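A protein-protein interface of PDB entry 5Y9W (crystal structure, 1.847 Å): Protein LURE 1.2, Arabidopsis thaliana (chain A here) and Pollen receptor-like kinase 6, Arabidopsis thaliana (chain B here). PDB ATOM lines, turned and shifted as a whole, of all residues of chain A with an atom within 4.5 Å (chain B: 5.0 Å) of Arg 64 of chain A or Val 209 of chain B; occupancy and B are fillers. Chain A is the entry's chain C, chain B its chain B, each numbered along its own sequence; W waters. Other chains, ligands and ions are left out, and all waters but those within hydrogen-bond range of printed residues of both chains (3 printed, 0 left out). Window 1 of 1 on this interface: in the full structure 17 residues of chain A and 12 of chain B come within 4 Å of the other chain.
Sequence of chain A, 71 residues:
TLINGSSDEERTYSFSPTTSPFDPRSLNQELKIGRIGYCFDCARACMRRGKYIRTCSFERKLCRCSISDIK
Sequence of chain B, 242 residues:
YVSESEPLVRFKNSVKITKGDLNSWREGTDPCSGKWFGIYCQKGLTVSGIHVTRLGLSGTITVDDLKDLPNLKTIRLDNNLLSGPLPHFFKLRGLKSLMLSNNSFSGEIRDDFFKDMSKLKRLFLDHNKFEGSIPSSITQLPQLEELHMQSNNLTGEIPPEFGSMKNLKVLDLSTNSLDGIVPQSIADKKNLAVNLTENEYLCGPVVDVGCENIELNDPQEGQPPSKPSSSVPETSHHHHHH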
ATOM      1  N   CYS A  42     -15.882  22.497 -11.890  1.00  0.00           N
ATOM      2  CA  CYS A  42     -15.934  21.540 -10.786  1.00  0.00           C
ATOM      3  C   CYS A  42     -17.289  20.842 -10.727  1.00  0.00           C
ATOM      4  O   CYS A  42     -17.359  19.615 -10.564  1.00  0.00           O
ATOM      5  CB  CYS A  42     -15.623  22.254  -9.463  1.00  0.00           C
ATOM      6  SG  CYS A  42     -15.654  21.197  -7.954  1.00  0.00           S
ATOM      7  N   CYS A  46     -17.921  16.705 -11.122  1.00  0.00           N
ATOM      8  CA  CYS A  46     -18.690  15.884 -10.193  1.00  0.00           C
ATOM      9  C   CYS A  46     -19.850  15.189 -10.896  1.00  0.00           C
ATOM     10  O   CYS A  46     -20.097  13.999 -10.665  1.00  0.00           O
ATOM     11  CB  CYS A  46     -19.188  16.743  -9.027  1.00  0.00           C
ATOM     12  SG  CYS A  46     -17.820  17.336  -7.987  1.00  0.00           S
ATOM     13  N   ILE A  53     -21.535  18.267  -6.425  1.00  0.00           N
ATOM     14  CA  ILE A  53     -20.440  19.117  -5.973  1.00  0.00           C
ATOM     15  C   ILE A  53     -20.635  19.411  -4.490  1.00  0.00           C
ATOM     16  O   ILE A  53     -21.764  19.631  -4.028  1.00  0.00           O
ATOM     17  CB  ILE A  53     -20.353  20.406  -6.814  1.00  0.00           C
ATOM     18  CG1 ILE A  53     -19.179  21.274  -6.341  1.00  0.00           C
ATOM     19  CG2 ILE A  53     -21.675  21.178  -6.800  1.00  0.00           C
ATOM     20  CD1 ILE A  53     -18.828  22.428  -7.277  1.00  0.00           C
ATOM     21  N   ARG A  54     -19.539  19.374  -3.722  1.00  0.00           N
ATOM     22  CA  ARG A  54     -19.572  19.646  -2.284  1.00  0.00           C
ATOM     23  C   ARG A  54     -18.685  20.802  -1.854  1.00  0.00           C
ATOM     24  O   ARG A  54     -19.089  21.602  -0.994  1.00  0.00           O
ATOM     25  CB  ARG A  54     -19.153  18.387  -1.489  1.00  0.00           C
ATOM     26  CG  ARG A  54     -20.219  17.302  -1.419  1.00  0.00           C
ATOM     27  CD  ARG A  54     -21.265  17.626  -0.371  1.00  0.00           C
ATOM     28  NE  ARG A  54     -22.347  16.638  -0.338  1.00  0.00           N
ATOM     29  CZ  ARG A  54     -23.521  16.806  -0.938  1.00  0.00           C
ATOM     30  NH1 ARG A  54     -23.761  17.912  -1.629  1.00  0.00           N
ATOM     31  NH2 ARG A  54     -24.455  15.872  -0.852  1.00  0.00           N
ATOM     32  N   THR A  55     -17.480  20.901  -2.408  1.00  0.00           N
ATOM     33  CA  THR A  55     -16.484  21.890  -2.014  1.00  0.00           C
ATOM     34  C   THR A  55     -15.832  22.448  -3.266  1.00  0.00           C
ATOM     35  O   THR A  55     -15.447  21.678  -4.149  1.00  0.00           O
ATOM     36  CB  THR A  55     -15.417  21.255  -1.119  1.00  0.00           C
ATOM     37  OG1 THR A  55     -16.065  20.489  -0.099  1.00  0.00           O
ATOM     38  CG2 THR A  55     -14.500  22.343  -0.484  1.00  0.00           C
ATOM     39  N   LEU A  62      -9.178  23.617  -5.247  1.00  0.00           N
ATOM     40  CA  LEU A  62      -9.767  22.449  -4.612  1.00  0.00           C
ATOM     41  C   LEU A  62     -11.165  22.202  -5.164  1.00  0.00           C
ATOM     42  O   LEU A  62     -12.017  23.097  -5.139  1.00  0.00           O
ATOM     43  CB  LEU A  62      -9.834  22.632  -3.092  1.00  0.00           C
ATOM     44  CG  LEU A  62     -10.486  21.441  -2.393  1.00  0.00           C
ATOM     45  CD1 LEU A  62      -9.665  20.145  -2.529  1.00  0.00           C
ATOM     46  CD2 LEU A  62     -10.762  21.732  -0.939  1.00  0.00           C
ATOM     47  N   CYS A  63     -11.404  20.977  -5.627  1.00  0.00           N
ATOM     48  CA  CYS A  63     -12.716  20.543  -6.090  1.00  0.00           C
ATOM     49  C   CYS A  63     -12.988  19.194  -5.452  1.00  0.00           C
ATOM     50  O   CYS A  63     -12.222  18.251  -5.668  1.00  0.00           O
ATOM     51  CB  CYS A  63     -12.751  20.428  -7.625  1.00  0.00           C
ATOM     52  SG  CYS A  63     -14.269  19.734  -8.282  1.00  0.00           S
ATOM     53  N   ARG A  64     -14.059  19.102  -4.659  1.00  0.00           N
ATOM     54  CA  ARG A  64     -14.460  17.845  -4.040  1.00  0.00           C
ATOM     55  C   ARG A  64     -15.926  17.579  -4.331  1.00  0.00           C
ATOM     56  O   ARG A  64     -16.747  18.503  -4.334  1.00  0.00           O
ATOM     57  CB  ARG A  64     -14.228  17.866  -2.513  1.00  0.00           C
ATOM     58  CG  ARG A  64     -12.771  17.800  -2.112  1.00  0.00           C
ATOM     59  CD  ARG A  64     -12.620  18.025  -0.611  1.00  0.00           C
ATOM     60  NE  ARG A  64     -11.283  17.681  -0.140  1.00  0.00           N
ATOM     61  CZ  ARG A  64     -10.805  17.985   1.061  1.00  0.00           C
ATOM     62  NH1 ARG A  64     -11.559  18.666   1.918  1.00  0.00           N
ATOM     63  NH2 ARG A  64      -9.573  17.606   1.411  1.00  0.00           N
ATOM     64  N   CYS A  65     -16.248  16.311  -4.569  1.00  0.00           N
ATOM     65  CA  CYS A  65     -17.612  15.861  -4.764  1.00  0.00           C
ATOM     66  C   CYS A  65     -18.085  15.048  -3.561  1.00  0.00           C
ATOM     67  O   CYS A  65     -17.309  14.665  -2.682  1.00  0.00           O
ATOM     68  CB  CYS A  65     -17.733  15.013  -6.041  1.00  0.00           C
ATOM     69  SG  CYS A  65     -16.811  15.637  -7.463  1.00  0.00           S
ATOM     70  N   SER A  66     -19.383  14.769  -3.560  1.00  0.00           N
ATOM     71  CA  SER A  66     -19.993  13.909  -2.561  1.00  0.00           C
ATOM     72  C   SER A  66     -19.528  12.463  -2.724  1.00  0.00           C
ATOM     73  O   SER A  66     -19.052  12.040  -3.782  1.00  0.00           O
ATOM     74  CB  SER A  66     -21.520  13.970  -2.666  1.00  0.00           C
ATOM     75  OG  SER A  66     -21.984  13.361  -3.869  1.00  0.00           O
ATOM     76  N   ILE A  67     -19.660  11.699  -1.642  1.00  0.00           N
ATOM     77  CA  ILE A  67     -19.510  10.251  -1.751  1.00  0.00           C
ATOM     78  C   ILE A  67     -20.814   9.603  -2.218  1.00  0.00           C
ATOM     79  O   ILE A  67     -20.781   8.615  -2.958  1.00  0.00           O
ATOM     80  CB  ILE A  67     -19.030   9.658  -0.416  1.00  0.00           C
ATOM     81  CG1 ILE A  67     -17.794  10.412   0.071  1.00  0.00           C
ATOM     82  CG2 ILE A  67     -18.701   8.177  -0.569  1.00  0.00           C
ATOM     83  CD1 ILE A  67     -17.356  10.052   1.474  1.00  0.00           C
ATOM     84  N   TYR B 201     -13.707  22.798   4.662  1.00  0.00           N
ATOM     85  CA  TYR B 201     -12.596  21.944   4.207  1.00  0.00           C
ATOM     86  C   TYR B 201     -12.559  20.586   4.891  1.00  0.00           C
ATOM     87  O   TYR B 201     -11.655  19.792   4.625  1.00  0.00           O
ATOM     88  CB  TYR B 201     -11.252  22.672   4.394  1.00  0.00           C
ATOM     89  CG  TYR B 201     -11.199  23.848   3.460  1.00  0.00           C
ATOM     90  CD1 TYR B 201     -10.746  23.704   2.143  1.00  0.00           C
ATOM     91  CD2 TYR B 201     -11.677  25.095   3.860  1.00  0.00           C
ATOM     92  CE1 TYR B 201     -10.745  24.796   1.270  1.00  0.00           C
ATOM     93  CE2 TYR B 201     -11.678  26.172   2.998  1.00  0.00           C
ATOM     94  CZ  TYR B 201     -11.211  26.019   1.706  1.00  0.00           C
ATOM     95  OH  TYR B 201     -11.223  27.125   0.865  1.00  0.00           O
ATOM     96  N   LEU B 202     -13.535  20.296   5.748  1.00  0.00           N
ATOM     97  CA  LEU B 202     -13.685  18.961   6.311  1.00  0.00           C
ATOM     98  C   LEU B 202     -14.219  17.986   5.259  1.00  0.00           C
ATOM     99  O   LEU B 202     -15.131  18.311   4.489  1.00  0.00           O
ATOM    100  CB  LEU B 202     -14.646  19.056   7.508  1.00  0.00           C
ATOM    101  CG  LEU B 202     -14.873  17.859   8.415  1.00  0.00           C
ATOM    102  CD1 LEU B 202     -13.575  17.403   9.011  1.00  0.00           C
ATOM    103  CD2 LEU B 202     -15.879  18.270   9.528  1.00  0.00           C
ATOM    104  N   CYS B 203     -13.669  16.774   5.228  1.00  0.00           N
ATOM    105  CA  CYS B 203     -14.143  15.766   4.294  1.00  0.00           C
ATOM    106  C   CYS B 203     -14.334  14.444   5.022  1.00  0.00           C
ATOM    107  O   CYS B 203     -13.908  14.264   6.165  1.00  0.00           O
ATOM    108  CB  CYS B 203     -13.169  15.585   3.107  1.00  0.00           C
ATOM    109  SG  CYS B 203     -11.488  15.066   3.481  1.00  0.00           S
ATOM    110  N   GLY B 204     -14.934  13.499   4.322  1.00  0.00           N
ATOM    111  CA  GLY B 204     -15.035  12.158   4.832  1.00  0.00           C
ATOM    112  C   GLY B 204     -16.477  11.742   5.022  1.00  0.00           C
ATOM    113  O   GLY B 204     -17.410  12.363   4.509  1.00  0.00           O
ATOM    114  N   VAL B 207     -19.851  13.993   6.720  1.00  0.00           N
ATOM    115  CA  VAL B 207     -20.203  15.178   5.945  1.00  0.00           C
ATOM    116  C   VAL B 207     -20.545  14.851   4.490  1.00  0.00           C
ATOM    117  O   VAL B 207     -20.903  15.758   3.728  1.00  0.00           O
ATOM    118  CB  VAL B 207     -19.038  16.188   6.011  1.00  0.00           C
ATOM    119  CG1 VAL B 207     -18.913  16.737   7.419  1.00  0.00           C
ATOM    120  CG2 VAL B 207     -17.755  15.508   5.618  1.00  0.00           C
ATOM    121  N   ASP B 208     -20.458  13.587   4.090  1.00  0.00           N
ATOM    122  CA  ASP B 208     -20.744  13.158   2.709  1.00  0.00           C
ATOM    123  C   ASP B 208     -19.865  13.901   1.695  1.00  0.00           C
ATOM    124  O   ASP B 208     -20.355  14.432   0.699  1.00  0.00           O
ATOM    125  CB  ASP B 208     -22.231  13.347   2.382  1.00  0.00           C
ATOM    126  CG  ASP B 208     -22.629  12.740   1.039  1.00  0.00           C
ATOM    127  OD1 ASP B 208     -21.943  11.811   0.589  1.00  0.00           O
ATOM    128  OD2 ASP B 208     -23.626  13.203   0.447  1.00  0.00           O
ATOM    129  N   VAL B 209     -18.555  13.950   1.957  1.00  0.00           N
ATOM    130  CA  VAL B 209     -17.617  14.667   1.086  1.00  0.00           C
ATOM    131  C   VAL B 209     -16.409  13.786   0.790  1.00  0.00           C
ATOM    132  O   VAL B 209     -15.643  13.440   1.700  1.00  0.00           O
ATOM    133  CB  VAL B 209     -17.151  16.004   1.695  1.00  0.00           C
ATOM    134  CG1 VAL B 209     -16.165  16.686   0.756  1.00  0.00           C
ATOM    135  CG2 VAL B 209     -18.326  16.924   1.997  1.00  0.00           C
ATOM    136  N   GLY B 210     -16.195  13.472  -0.488  1.00  0.00           N
ATOM    137  CA  GLY B 210     -14.996  12.742  -0.866  1.00  0.00           C
ATOM    138  C   GLY B 210     -13.756  13.599  -0.687  1.00  0.00           C
ATOM    139  O   GLY B 210     -13.703  14.747  -1.144  1.00  0.00           O
ATOM    140  N   CYS B 211     -12.733  13.036  -0.040  1.00  0.00           N
ATOM    141  CA  CYS B 211     -11.546  13.829   0.250  1.00  0.00           C
ATOM    142  C   CYS B 211     -10.756  14.167  -1.004  1.00  0.00           C
ATOM    143  O   CYS B 211     -10.039  15.172  -1.020  1.00  0.00           O
ATOM    144  CB  CYS B 211     -10.648  13.101   1.248  1.00  0.00           C
ATOM    145  SG  CYS B 211     -11.374  13.090   2.937  1.00  0.00           S
ATOM    146  N   GLU B 212     -10.864  13.347  -2.050  1.00  0.00           N
ATOM    147  CA  GLU B 212     -10.000  13.518  -3.211  1.00  0.00           C
ATOM    148  C   GLU B 212     -10.234  14.867  -3.877  1.00  0.00           C
ATOM    149  O   GLU B 212     -11.371  15.255  -4.147  1.00  0.00           O
ATOM    150  CB  GLU B 212     -10.233  12.402  -4.225  1.00  0.00           C
ATOM    151  CG  GLU B 212      -9.392  12.583  -5.478  1.00  0.00           C
ATOM    152  CD  GLU B 212      -9.625  11.501  -6.506  1.00  0.00           C
ATOM    153  OE1 GLU B 212      -8.745  11.329  -7.376  1.00  0.00           O
ATOM    154  OE2 GLU B 212     -10.677  10.826  -6.449  1.00  0.00           O
ATOM    155  N   ASN B 213      -9.147  15.573  -4.143  1.00  0.00           N
ATOM    156  CA  ASN B 213      -9.190  16.811  -4.910  1.00  0.00           C
ATOM    157  C   ASN B 213      -9.253  16.441  -6.390  1.00  0.00           C
ATOM    158  O   ASN B 213      -8.310  15.852  -6.915  1.00  0.00           O
ATOM    159  CB  ASN B 213      -7.959  17.657  -4.596  1.00  0.00           C
ATOM    160  CG  ASN B 213      -7.953  18.991  -5.319  1.00  0.00           C
ATOM    161  OD1 ASN B 213      -8.921  19.367  -5.985  1.00  0.00           O
ATOM    162  ND2 ASN B 213      -6.856  19.717  -5.186  1.00  0.00           N
ATOM    163  N   ILE B 214     -10.377  16.738  -7.043  1.00  0.00           N
ATOM    164  CA  ILE B 214     -10.534  16.528  -8.485  1.00  0.00           C
ATOM    165  C   ILE B 214      -9.858  17.684  -9.215  1.00  0.00           C
ATOM    166  O   ILE B 214     -10.273  18.839  -9.082  1.00  0.00           O
ATOM    167  CB  ILE B 214     -12.018  16.445  -8.879  1.00  0.00           C
ATOM    168  CG1 ILE B 214     -12.827  15.598  -7.888  1.00  0.00           C
ATOM    169  CG2 ILE B 214     -12.167  15.944 -10.317  1.00  0.00           C
ATOM    170  CD1 ILE B 214     -12.357  14.178  -7.733  1.00  0.00           C
HETATM  171  O   HOH W   1     -14.125  14.534  -3.910  1.00  0.00           O
HETATM  172  O   HOH W   2     -14.473  19.632   2.015  1.00  0.00           O
HETATM  173  O   HOH W   3      -7.440  17.316  -0.897  1.00  0.00           O
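Water W2 lies within hydrogen-bond range of OG1 of Thr 55 of chain A, O of Leu 202 of chain B and NH1 of Arg 64 of chain A.
Water W1 lies within hydrogen-bond range of the backbone carbonyl oxygen of Gly 210 of chain B (2.8 Å), the backbone NH of Cys 65 of chain A (2.8 Å) and the backbone carbonyl oxygen of Glu 212 of chain B (2.9 Å).
Water W3 bridges the guanidinium group of Arg 64 of chain A (3.2 Å) and the backbone carbonyl oxygen of Cys 211 of chain B (3.4 Å).
The side-chain sulfur (SG) of Cys 203 of chain B is disulfide-bonded to the side-chain sulfur (SG) of Cys 211 of chain B.
The backbone carbonyl oxygen (O) of Val 209 of chain B is in hydrogen-bond range of the backbone NH (N) of Gly 204 of chain B, at 2.7 Å.
SG of Cys 63 of chain A forms a disulfide with SG of Cys 42 of chain A (2.0 Å).
SG of Cys 65 of chain A is disulfide-bonded to SG of Cys 46 of chain A, at 2.0 Å.
The backbone carbonyl oxygen (O) of Arg 64 of chain A lies within hydrogen-bond range of the backbone NH (N) of Arg 54 of chain A.
The backbone carbonyl oxygen (O) of Thr 55 of chain A lies within hydrogen-bond range of the backbone NH (N) of Arg 64 of chain A.
Arg 54 of chain A touches Val 209 of chain B.
Thr 55 of chain A touches Val 209 of chain B (OG1 to CG1, 3.9 Å).
Asn 213 of chain B touches Leu 62 of chain A.
Val 209 of chain B touches Arg 64 of chain A.
Arg 64 of chain A touches Gly 210 of chain B.
CG of Arg 64 of chain A touches O of Glu 212 of chain B (3.5 Å).
Cys 65 of chain A touches Val 209 of chain B (O to C, 3.7 Å).
Asp 208 of chain B touches Ser 66 of chain A.
Ile 67 of chain A touches Gly 204 of chain B.
Ile 67 of chain A touches Gly 210 of chain B (CG1 to N, 3.5 Å).
O of Tyr 201 of chain B lies within hydrogen-bond range of NH1 of Arg 64 of chain A.
NH2 of Arg 64 of chain A lies within hydrogen-bond range of SG of Cys 203 of chain B, at 3.8 Å.
OD2 of Asp 208 of chain B lies within salt-bridge range of NH2 of Arg 54 of chain A (3.1 Å).
The side-chain carboxylate (OD1) of Asp 208 of chain B lies within hydrogen-bond range of the backbone NH (N) of Ile 67 of chain A, 3.2 Å away.
The backbone NH (N) of Gly 210 of chain B sits at hydrogen-bond distance from the backbone carbonyl oxygen (O) of Cys 65 of chain A, 2.7 Å away.
The backbone carbonyl oxygen (O) of Cys 211 of chain B lies within hydrogen-bond range of the guanidinium group (NE) of Arg 64 of chain A.
The side-chain amide oxygen (OD1) of Asn 213 of chain B sits at hydrogen-bond distance from the backbone NH (N) of Cys 63 of chain A (3.0 Å).
The backbone NH (N) of Ile 214 of chain B is in hydrogen-bond range of the backbone carbonyl oxygen (O) of Cys 63 of chain A.
O of Glu 212 of chain B lies close to O of Cys 63 of chain A (3.5 Å).
Arg 64 of chain A touches just these residues of chain B: Tyr 201 (2.9 Å), Cys 203 (3.7 Å), Val 209 (3.98 Å), Gly 210 (3.3 Å), Cys 211 (2.9 Å) and Glu 212 (3.5 Å).
Of the printed residues of chain A, Tyr 201 of chain B touches Leu 62 (3.7 Å) and Arg 64 (2.9 Å).
Of the printed residues of chain A, Cys 211 of chain B touches Arg 64 (2.9 Å).
Of the printed residues of chain B, Ser 66 of chain A touches Asp 208.
Of the printed residues of chain A, Gly 210 of chain B touches Arg 64, Cys 65 and Ile 67.
Printed residues of chain B within 4 Å of Ile 67 of chain A: Gly 204 (3.8 Å), Asp 208 (3.2 Å), Val 209 (3.7 Å) and Gly 210 (3.5 Å).
Cys 46 of chain A touches none of the printed residues of chain B.
Leu 202 of chain B touches none of the printed residues of chain A.
The nearest printed residue of chain A that does not touch Asn 213 of chain B is Arg 64 of chain A (4.7 Å).
Of the 12 printed residues of chain B, 10 touch a printed residue of chain A.
Hydrophobic or aromatic side chains of chain B that line the printed part of chain A: Tyr 201, Val 209 and Ile 214.
Printed residues of chain A that touch a printed residue of chain B: Arg 54, Thr 55, Leu 62, Cys 63, Arg 64, Cys 65, Ser 66 and Ile 67.
Hydrophobic or aromatic side chains of chain A that line the printed part of chain B: Leu 62 and Ile 67.
Among the printed residues, 21 pairs touch across the chains.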
